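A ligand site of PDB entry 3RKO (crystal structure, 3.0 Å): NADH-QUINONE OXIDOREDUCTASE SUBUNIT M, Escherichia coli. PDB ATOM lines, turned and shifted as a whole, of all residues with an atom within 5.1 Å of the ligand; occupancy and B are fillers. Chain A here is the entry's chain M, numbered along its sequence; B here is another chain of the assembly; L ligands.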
ATOM      1  N   PHE A 306      32.257 -13.368   3.910  1.00  0.00           N
ATOM      2  CA  PHE A 306      31.480 -12.571   2.981  1.00  0.00           C
ATOM      3  C   PHE A 306      31.096 -11.227   3.582  1.00  0.00           C
ATOM      4  O   PHE A 306      31.119 -10.212   2.903  1.00  0.00           O
ATOM      5  CB  PHE A 306      30.234 -13.354   2.557  1.00  0.00           C
ATOM      6  CG  PHE A 306      29.095 -12.487   2.102  1.00  0.00           C
ATOM      7  CD1 PHE A 306      29.069 -11.984   0.813  1.00  0.00           C
ATOM      8  CD2 PHE A 306      28.053 -12.205   2.964  1.00  0.00           C
ATOM      9  CE1 PHE A 306      28.019 -11.193   0.397  1.00  0.00           C
ATOM     10  CE2 PHE A 306      26.996 -11.418   2.554  1.00  0.00           C
ATOM     11  CZ  PHE A 306      26.976 -10.912   1.259  1.00  0.00           C
ATOM     12  N   MET A 374      37.234   0.942  -3.084  1.00  0.00           N
ATOM     13  CA  MET A 374      37.778   0.438  -4.329  1.00  0.00           C
ATOM     14  C   MET A 374      36.675  -0.247  -5.126  1.00  0.00           C
ATOM     15  O   MET A 374      35.870  -1.001  -4.585  1.00  0.00           O
ATOM     16  CB  MET A 374      38.926  -0.546  -4.056  1.00  0.00           C
ATOM     17  CG  MET A 374      38.511  -1.706  -3.163  1.00  0.00           C
ATOM     18  SD  MET A 374      39.872  -2.688  -2.468  1.00  0.00           S
ATOM     19  CE  MET A 374      40.670  -3.291  -3.964  1.00  0.00           C
ATOM     20  N   GLY A 375      36.652   0.016  -6.431  1.00  0.00           N
ATOM     21  CA  GLY A 375      35.661  -0.578  -7.305  1.00  0.00           C
ATOM     22  C   GLY A 375      36.097  -0.381  -8.729  1.00  0.00           C
ATOM     23  O   GLY A 375      37.114   0.278  -8.978  1.00  0.00           O
ATOM     24  N   VAL A 430      28.038 -23.917  -2.240  1.00  0.00           N
ATOM     25  CA  VAL A 430      27.194 -22.824  -2.755  1.00  0.00           C
ATOM     26  C   VAL A 430      27.506 -21.473  -2.097  1.00  0.00           C
ATOM     27  O   VAL A 430      27.551 -20.436  -2.785  1.00  0.00           O
ATOM     28  CB  VAL A 430      25.699 -23.122  -2.622  1.00  0.00           C
ATOM     29  CG1 VAL A 430      24.936 -22.308  -3.641  1.00  0.00           C
ATOM     30  CG2 VAL A 430      25.422 -24.600  -2.815  1.00  0.00           C
ATOM     31  N   PHE A 431      27.711 -21.458  -0.782  1.00  0.00           N
ATOM     32  CA  PHE A 431      28.147 -20.218  -0.116  1.00  0.00           C
ATOM     33  C   PHE A 431      29.485 -19.703  -0.632  1.00  0.00           C
ATOM     34  O   PHE A 431      29.706 -18.490  -0.744  1.00  0.00           O
ATOM     35  CB  PHE A 431      28.256 -20.411   1.387  1.00  0.00           C
ATOM     36  CG  PHE A 431      26.920 -20.418   2.084  1.00  0.00           C
ATOM     37  CD1 PHE A 431      25.874 -21.170   1.597  1.00  0.00           C
ATOM     38  CD2 PHE A 431      26.731 -19.680   3.247  1.00  0.00           C
ATOM     39  CE1 PHE A 431      24.657 -21.183   2.246  1.00  0.00           C
ATOM     40  CE2 PHE A 431      25.521 -19.692   3.904  1.00  0.00           C
ATOM     41  CZ  PHE A 431      24.475 -20.442   3.403  1.00  0.00           C
ATOM     42  N   VAL A 434      28.992 -17.395  -3.411  1.00  0.00           N
ATOM     43  CA  VAL A 434      28.698 -16.044  -2.901  1.00  0.00           C
ATOM     44  C   VAL A 434      29.924 -15.247  -2.491  1.00  0.00           C
ATOM     45  O   VAL A 434      30.213 -14.202  -3.069  1.00  0.00           O
ATOM     46  CB  VAL A 434      27.765 -16.065  -1.667  1.00  0.00           C
ATOM     47  CG1 VAL A 434      27.855 -14.752  -0.876  1.00  0.00           C
ATOM     48  CG2 VAL A 434      26.346 -16.321  -2.073  1.00  0.00           C
ATOM     49  N   ALA A 438      31.316 -11.937  -4.380  1.00  0.00           N
ATOM     50  CA  ALA A 438      31.256 -10.658  -3.674  1.00  0.00           C
ATOM     51  C   ALA A 438      32.631  -9.991  -3.659  1.00  0.00           C
ATOM     52  O   ALA A 438      32.811  -8.883  -4.158  1.00  0.00           O
ATOM     53  CB  ALA A 438      30.731 -10.850  -2.250  1.00  0.00           C
ATOM     54  N   HIS A 441      33.626  -8.759  -7.184  1.00  0.00           N
ATOM     55  CA  HIS A 441      32.893  -7.537  -7.532  1.00  0.00           C
ATOM     56  C   HIS A 441      33.453  -6.338  -6.796  1.00  0.00           C
ATOM     57  O   HIS A 441      33.977  -5.392  -7.412  1.00  0.00           O
ATOM     58  CB  HIS A 441      31.411  -7.697  -7.210  1.00  0.00           C
ATOM     59  CG  HIS A 441      30.652  -8.442  -8.259  1.00  0.00           C
ATOM     60  ND1 HIS A 441      31.121  -8.588  -9.548  1.00  0.00           N
ATOM     61  CD2 HIS A 441      29.464  -9.099  -8.212  1.00  0.00           C
ATOM     62  CE1 HIS A 441      30.250  -9.292 -10.248  1.00  0.00           C
ATOM     63  NE2 HIS A 441      29.245  -9.612  -9.463  1.00  0.00           N
ATOM     64  N   ARG A 442      33.343  -6.354  -5.472  1.00  0.00           N
ATOM     65  CA  ARG A 442      33.817  -5.258  -4.652  1.00  0.00           C
ATOM     66  C   ARG A 442      35.166  -4.764  -5.135  1.00  0.00           C
ATOM     67  O   ARG A 442      35.387  -3.569  -5.192  1.00  0.00           O
ATOM     68  CB  ARG A 442      33.925  -5.690  -3.187  1.00  0.00           C
ATOM     69  CG  ARG A 442      32.599  -6.115  -2.548  1.00  0.00           C
ATOM     70  CD  ARG A 442      32.850  -7.309  -1.642  1.00  0.00           C
ATOM     71  NE  ARG A 442      31.635  -7.874  -1.080  1.00  0.00           N
ATOM     72  CZ  ARG A 442      31.291  -7.781   0.204  1.00  0.00           C
ATOM     73  NH1 ARG A 442      32.093  -7.137   1.054  1.00  0.00           N
ATOM     74  NH2 ARG A 442      30.168  -8.335   0.647  1.00  0.00           N
ATOM     75  N   PHE A 445      34.677  -4.759 -10.058  1.00  0.00           N
ATOM     76  CA  PHE A 445      33.490  -4.405 -10.836  1.00  0.00           C
ATOM     77  C   PHE A 445      32.654  -3.313 -10.180  1.00  0.00           C
ATOM     78  O   PHE A 445      32.556  -3.225  -8.960  1.00  0.00           O
ATOM     79  CB  PHE A 445      32.617  -5.637 -11.074  1.00  0.00           C
ATOM     80  CG  PHE A 445      33.331  -6.758 -11.761  1.00  0.00           C
ATOM     81  CD1 PHE A 445      34.430  -6.502 -12.576  1.00  0.00           C
ATOM     82  CD2 PHE A 445      32.916  -8.063 -11.602  1.00  0.00           C
ATOM     83  CE1 PHE A 445      35.095  -7.530 -13.210  1.00  0.00           C
ATOM     84  CE2 PHE A 445      33.575  -9.093 -12.243  1.00  0.00           C
ATOM     85  CZ  PHE A 445      34.676  -8.826 -13.050  1.00  0.00           C
ATOM     86  N   GLY A 446      32.055  -2.459 -11.012  1.00  0.00           N
ATOM     87  CA  GLY A 446      31.104  -1.485 -10.535  1.00  0.00           C
ATOM     88  C   GLY A 446      31.582  -0.052 -10.704  1.00  0.00           C
ATOM     89  O   GLY A 446      32.382   0.245 -11.598  1.00  0.00           O
ATOM     90  N   LYS A 447      31.085   0.825  -9.835  1.00  0.00           N
ATOM     91  CA  LYS A 447      31.509   2.224  -9.820  1.00  0.00           C
ATOM     92  C   LYS A 447      33.023   2.356  -9.870  1.00  0.00           C
ATOM     93  O   LYS A 447      33.734   1.742  -9.069  1.00  0.00           O
ATOM     94  CB  LYS A 447      30.958   2.923  -8.574  1.00  0.00           C
ATOM     95  CG  LYS A 447      31.180   2.136  -7.305  1.00  0.00           C
ATOM     96  CD  LYS A 447      30.465   2.767  -6.114  1.00  0.00           C
ATOM     97  CE  LYS A 447      30.565   1.865  -4.896  1.00  0.00           C
ATOM     98  NZ  LYS A 447      29.940   2.480  -3.691  1.00  0.00           N
ATOM     99  N   TYR B 158      30.352  -4.611 -16.724  1.00  0.00           N
ATOM    100  CA  TYR B 158      30.468  -4.476 -15.269  1.00  0.00           C
ATOM    101  C   TYR B 158      30.121  -3.103 -14.675  1.00  0.00           C
ATOM    102  O   TYR B 158      29.544  -3.047 -13.590  1.00  0.00           O
ATOM    103  CB  TYR B 158      31.838  -4.959 -14.761  1.00  0.00           C
ATOM    104  CG  TYR B 158      33.033  -4.285 -15.394  1.00  0.00           C
ATOM    105  CD1 TYR B 158      33.533  -4.721 -16.632  1.00  0.00           C
ATOM    106  CD2 TYR B 158      33.690  -3.239 -14.760  1.00  0.00           C
ATOM    107  CE1 TYR B 158      34.629  -4.109 -17.205  1.00  0.00           C
ATOM    108  CE2 TYR B 158      34.796  -2.635 -15.326  1.00  0.00           C
ATOM    109  CZ  TYR B 158      35.264  -3.075 -16.553  1.00  0.00           C
ATOM    110  OH  TYR B 158      36.358  -2.474 -17.135  1.00  0.00           O
ATOM    111  N   PRO B 161      25.897  -1.702 -11.718  1.00  0.00           N
ATOM    112  CA  PRO B 161      25.478  -2.561 -10.584  1.00  0.00           C
ATOM    113  C   PRO B 161      24.401  -3.609 -10.911  1.00  0.00           C
ATOM    114  O   PRO B 161      24.547  -4.778 -10.536  1.00  0.00           O
ATOM    115  CB  PRO B 161      24.919  -1.551  -9.584  1.00  0.00           C
ATOM    116  CG  PRO B 161      25.734  -0.332  -9.828  1.00  0.00           C
ATOM    117  CD  PRO B 161      26.006  -0.290 -11.313  1.00  0.00           C
ATOM    118  N   ALA B 165      24.746  -7.726 -10.746  1.00  0.00           N
ATOM    119  CA  ALA B 165      23.871  -8.505  -9.884  1.00  0.00           C
ATOM    120  C   ALA B 165      23.012  -9.513 -10.667  1.00  0.00           C
ATOM    121  O   ALA B 165      22.592 -10.545 -10.135  1.00  0.00           O
ATOM    122  CB  ALA B 165      23.004  -7.616  -9.025  1.00  0.00           C
ATOM    123  N   MET B 168      25.283 -12.416 -11.077  1.00  0.00           N
ATOM    124  CA  MET B 168      25.421 -13.128  -9.825  1.00  0.00           C
ATOM    125  C   MET B 168      24.175 -13.956  -9.487  1.00  0.00           C
ATOM    126  O   MET B 168      24.289 -15.066  -8.976  1.00  0.00           O
ATOM    127  CB  MET B 168      25.758 -12.175  -8.689  1.00  0.00           C
ATOM    128  CG  MET B 168      25.872 -12.864  -7.350  1.00  0.00           C
ATOM    129  SD  MET B 168      26.587 -11.813  -6.070  1.00  0.00           S
ATOM    130  CE  MET B 168      26.066 -12.713  -4.613  1.00  0.00           C
ATOM    131  N   VAL B 172      24.812 -17.907  -8.866  1.00  0.00           N
ATOM    132  CA  VAL B 172      24.249 -18.541  -7.673  1.00  0.00           C
ATOM    133  C   VAL B 172      23.258 -19.638  -8.015  1.00  0.00           C
ATOM    134  O   VAL B 172      23.393 -20.775  -7.564  1.00  0.00           O
ATOM    135  CB  VAL B 172      23.568 -17.536  -6.721  1.00  0.00           C
ATOM    136  CG1 VAL B 172      22.466 -18.221  -5.916  1.00  0.00           C
ATOM    137  CG2 VAL B 172      24.598 -16.884  -5.814  1.00  0.00           C
ATOM    138  N   VAL B 176      23.388 -23.719  -7.375  1.00  0.00           N
ATOM    139  CA  VAL B 176      22.515 -24.578  -6.562  1.00  0.00           C
ATOM    140  C   VAL B 176      22.076 -25.791  -7.382  1.00  0.00           C
ATOM    141  O   VAL B 176      22.087 -26.954  -6.910  1.00  0.00           O
ATOM    142  CB  VAL B 176      21.304 -23.816  -6.027  1.00  0.00           C
ATOM    143  CG1 VAL B 176      20.504 -24.683  -5.065  1.00  0.00           C
ATOM    144  CG2 VAL B 176      21.769 -22.568  -5.321  1.00  0.00           C
ATOM    145  N   PHE B 549      15.100 -16.763   1.320  1.00  0.00           N
ATOM    146  CA  PHE B 549      16.524 -17.097   1.232  1.00  0.00           C
ATOM    147  C   PHE B 549      17.428 -15.876   1.399  1.00  0.00           C
ATOM    148  O   PHE B 549      18.089 -15.712   2.426  1.00  0.00           O
ATOM    149  CB  PHE B 549      16.850 -17.788  -0.091  1.00  0.00           C
ATOM    150  CG  PHE B 549      16.126 -19.089  -0.297  1.00  0.00           C
ATOM    151  CD1 PHE B 549      15.866 -19.551  -1.579  1.00  0.00           C
ATOM    152  CD2 PHE B 549      15.700 -19.836   0.783  1.00  0.00           C
ATOM    153  CE1 PHE B 549      15.200 -20.741  -1.763  1.00  0.00           C
ATOM    154  CE2 PHE B 549      15.034 -21.026   0.599  1.00  0.00           C
ATOM    155  CZ  PHE B 549      14.780 -21.486  -0.675  1.00  0.00           C
ATOM    156  N   VAL B 550      17.468 -15.044   0.369  1.00  0.00           N
ATOM    157  CA  VAL B 550      18.383 -13.905   0.344  1.00  0.00           C
ATOM    158  C   VAL B 550      18.270 -13.034   1.600  1.00  0.00           C
ATOM    159  O   VAL B 550      19.272 -12.753   2.267  1.00  0.00           O
ATOM    160  CB  VAL B 550      18.164 -13.050  -0.928  1.00  0.00           C
ATOM    161  CG1 VAL B 550      19.127 -11.880  -0.943  1.00  0.00           C
ATOM    162  CG2 VAL B 550      18.326 -13.911  -2.170  1.00  0.00           C
ATOM    163  N   PHE B 553      19.513 -14.917   4.736  1.00  0.00           N
ATOM    164  CA  PHE B 553      20.941 -15.187   4.593  1.00  0.00           C
ATOM    165  C   PHE B 553      21.756 -13.949   4.935  1.00  0.00           C
ATOM    166  O   PHE B 553      22.652 -13.980   5.794  1.00  0.00           O
ATOM    167  CB  PHE B 553      21.267 -15.634   3.158  1.00  0.00           C
ATOM    168  CG  PHE B 553      22.665 -15.289   2.722  1.00  0.00           C
ATOM    169  CD1 PHE B 553      23.719 -16.127   2.994  1.00  0.00           C
ATOM    170  CD2 PHE B 553      22.906 -14.110   2.038  1.00  0.00           C
ATOM    171  CE1 PHE B 553      25.004 -15.804   2.594  1.00  0.00           C
ATOM    172  CE2 PHE B 553      24.191 -13.786   1.638  1.00  0.00           C
ATOM    173  CZ  PHE B 553      25.249 -14.634   1.910  1.00  0.00           C
ATOM    174  N   LEU B 554      21.431 -12.847   4.252  1.00  0.00           N
ATOM    175  CA  LEU B 554      22.065 -11.560   4.527  1.00  0.00           C
ATOM    176  C   LEU B 554      21.804 -11.174   5.966  1.00  0.00           C
ATOM    177  O   LEU B 554      22.615 -10.489   6.600  1.00  0.00           O
ATOM    178  CB  LEU B 554      21.525 -10.480   3.592  1.00  0.00           C
ATOM    179  CG  LEU B 554      21.702 -10.643   2.080  1.00  0.00           C
ATOM    180  CD1 LEU B 554      21.014  -9.511   1.355  1.00  0.00           C
ATOM    181  CD2 LEU B 554      23.174 -10.722   1.691  1.00  0.00           C
HETATM  182  C1  LIG L   1      29.965  -4.923  -5.093  1.00  0.00           C
HETATM  183  O1  LIG L   1      28.721  -4.603  -4.480  1.00  0.00           O
HETATM  184  C2  LIG L   1      30.849  -3.679  -5.004  1.00  0.00           C
HETATM  185  O2  LIG L   1      31.042  -3.313  -3.628  1.00  0.00           O
HETATM  186  C3  LIG L   1      30.296  -2.488  -5.714  1.00  0.00           C
HETATM  187  O3  LIG L   1      31.203  -1.429  -5.565  1.00  0.00           O
HETATM  188  C4  LIG L   1      30.031  -2.823  -7.157  1.00  0.00           C
HETATM  189  O4  LIG L   1      29.479  -1.764  -7.866  1.00  0.00           O
HETATM  190  C5  LIG L   1      29.145  -4.047  -7.236  1.00  0.00           C
HETATM  191  O5  LIG L   1      29.681  -5.163  -6.479  1.00  0.00           O
HETATM  192  C6  LIG L   1      28.823  -4.334  -8.647  1.00  0.00           C
HETATM  193  O6  LIG L   1      30.005  -4.716  -9.340  1.00  0.00           O
HETATM  194  O7  LIG L   1      28.024  -6.529  -0.664  1.00  0.00           O
HETATM  195  O8  LIG L   1      26.494  -8.559  -6.277  1.00  0.00           O
HETATM  196  O9  LIG L   1      26.919  -5.902  -6.473  1.00  0.00           O
HETATM  197  C7  LIG L   1      23.074 -12.554  -1.856  1.00  0.00           C
HETATM  198  C8  LIG L   1      23.653 -11.145  -1.617  1.00  0.00           C
HETATM  199  C9  LIG L   1      24.072 -13.659  -1.687  1.00  0.00           C
HETATM  200  C10 LIG L   1      21.487 -19.725  -0.478  1.00  0.00           C
HETATM  201  C11 LIG L   1      24.813 -10.954  -2.588  1.00  0.00           C
HETATM  202  C12 LIG L   1      23.462 -15.057  -1.956  1.00  0.00           C
HETATM  203  C13 LIG L   1      20.268 -18.781  -0.677  1.00  0.00           C
HETATM  204  C14 LIG L   1      22.556 -19.313  -1.516  1.00  0.00           C
HETATM  205  C15 LIG L   1      25.488  -9.574  -2.676  1.00  0.00           C
HETATM  206  C16 LIG L   1      27.885  -5.849  -1.921  1.00  0.00           C
HETATM  207  C17 LIG L   1      22.301 -15.462  -1.040  1.00  0.00           C
HETATM  208  C18 LIG L   1      20.727 -17.350  -0.331  1.00  0.00           C
HETATM  209  C19 LIG L   1      23.017 -17.880  -1.184  1.00  0.00           C
HETATM  210  O10 LIG L   1      27.589  -7.818  -2.876  1.00  0.00           O
HETATM  211  O11 LIG L   1      26.568  -9.808  -3.613  1.00  0.00           O
HETATM  212  C20 LIG L   1      21.827 -16.895  -1.338  1.00  0.00           C
HETATM  213  C21 LIG L   1      28.405  -6.685  -3.141  1.00  0.00           C
HETATM  214  C22 LIG L   1      26.708  -7.787  -5.100  1.00  0.00           C
HETATM  215  C23 LIG L   1      27.601  -6.619  -5.453  1.00  0.00           C
HETATM  216  C24 LIG L   1      27.379  -8.673  -4.000  1.00  0.00           C
HETATM  217  C25 LIG L   1      27.871  -5.753  -4.200  1.00  0.00           C
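The guanidinium group (NH2) of Arg 442 is in hydrogen-bond range of an oxygen (O7) of the ligand. The backbone carbonyl oxygen (O) of Phe 445 sits at hydrogen-bond distance from an oxygen (O6) of the ligand. N of Gly 446 lies within hydrogen-bond range of O6 of the ligand (3.5 Å). An oxygen (O8) of the ligand lies within hydrogen-bond range of the side-chain sulfur (SD) of Met 168 of chain B (3.3 Å).
The backbone carbonyl oxygen of Arg 442 sits close to the backbone carbonyl oxygen of Met 374. The guanidinium group of Arg 442 sits at hydrogen-bond distance from the backbone carbonyl oxygen of Phe 306. The backbone carbonyl oxygen (O) of Ala 438 sits close to the guanidinium group (NE) of Arg 442.
Merely in contact with the ligand: Val 434 (3.2 Å), His 441 (3.2 Å), Lys 447 (3.4 Å), Phe 549 of chain B (3.6 Å), Phe 553 of chain B (3.3 Å) and Leu 554 of chain B (3.4 Å). Hydrophobic or aromatic side chains that line the ligand: Val 434, His 441, Phe 445, Met 168 of chain B, Phe 549 of chain B, Phe 553 of chain B and Leu 554 of chain B. Within 4 Å of the ligand: Val 434, His 441, Arg 442, Phe 445, Gly 446, Lys 447, Met 168 of chain B, Phe 549 of chain B, Phe 553 of chain B and Leu 554 of chain B. The nearest printed residue that does not touch the ligand is Val 550 of chain B (4.1 Å).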
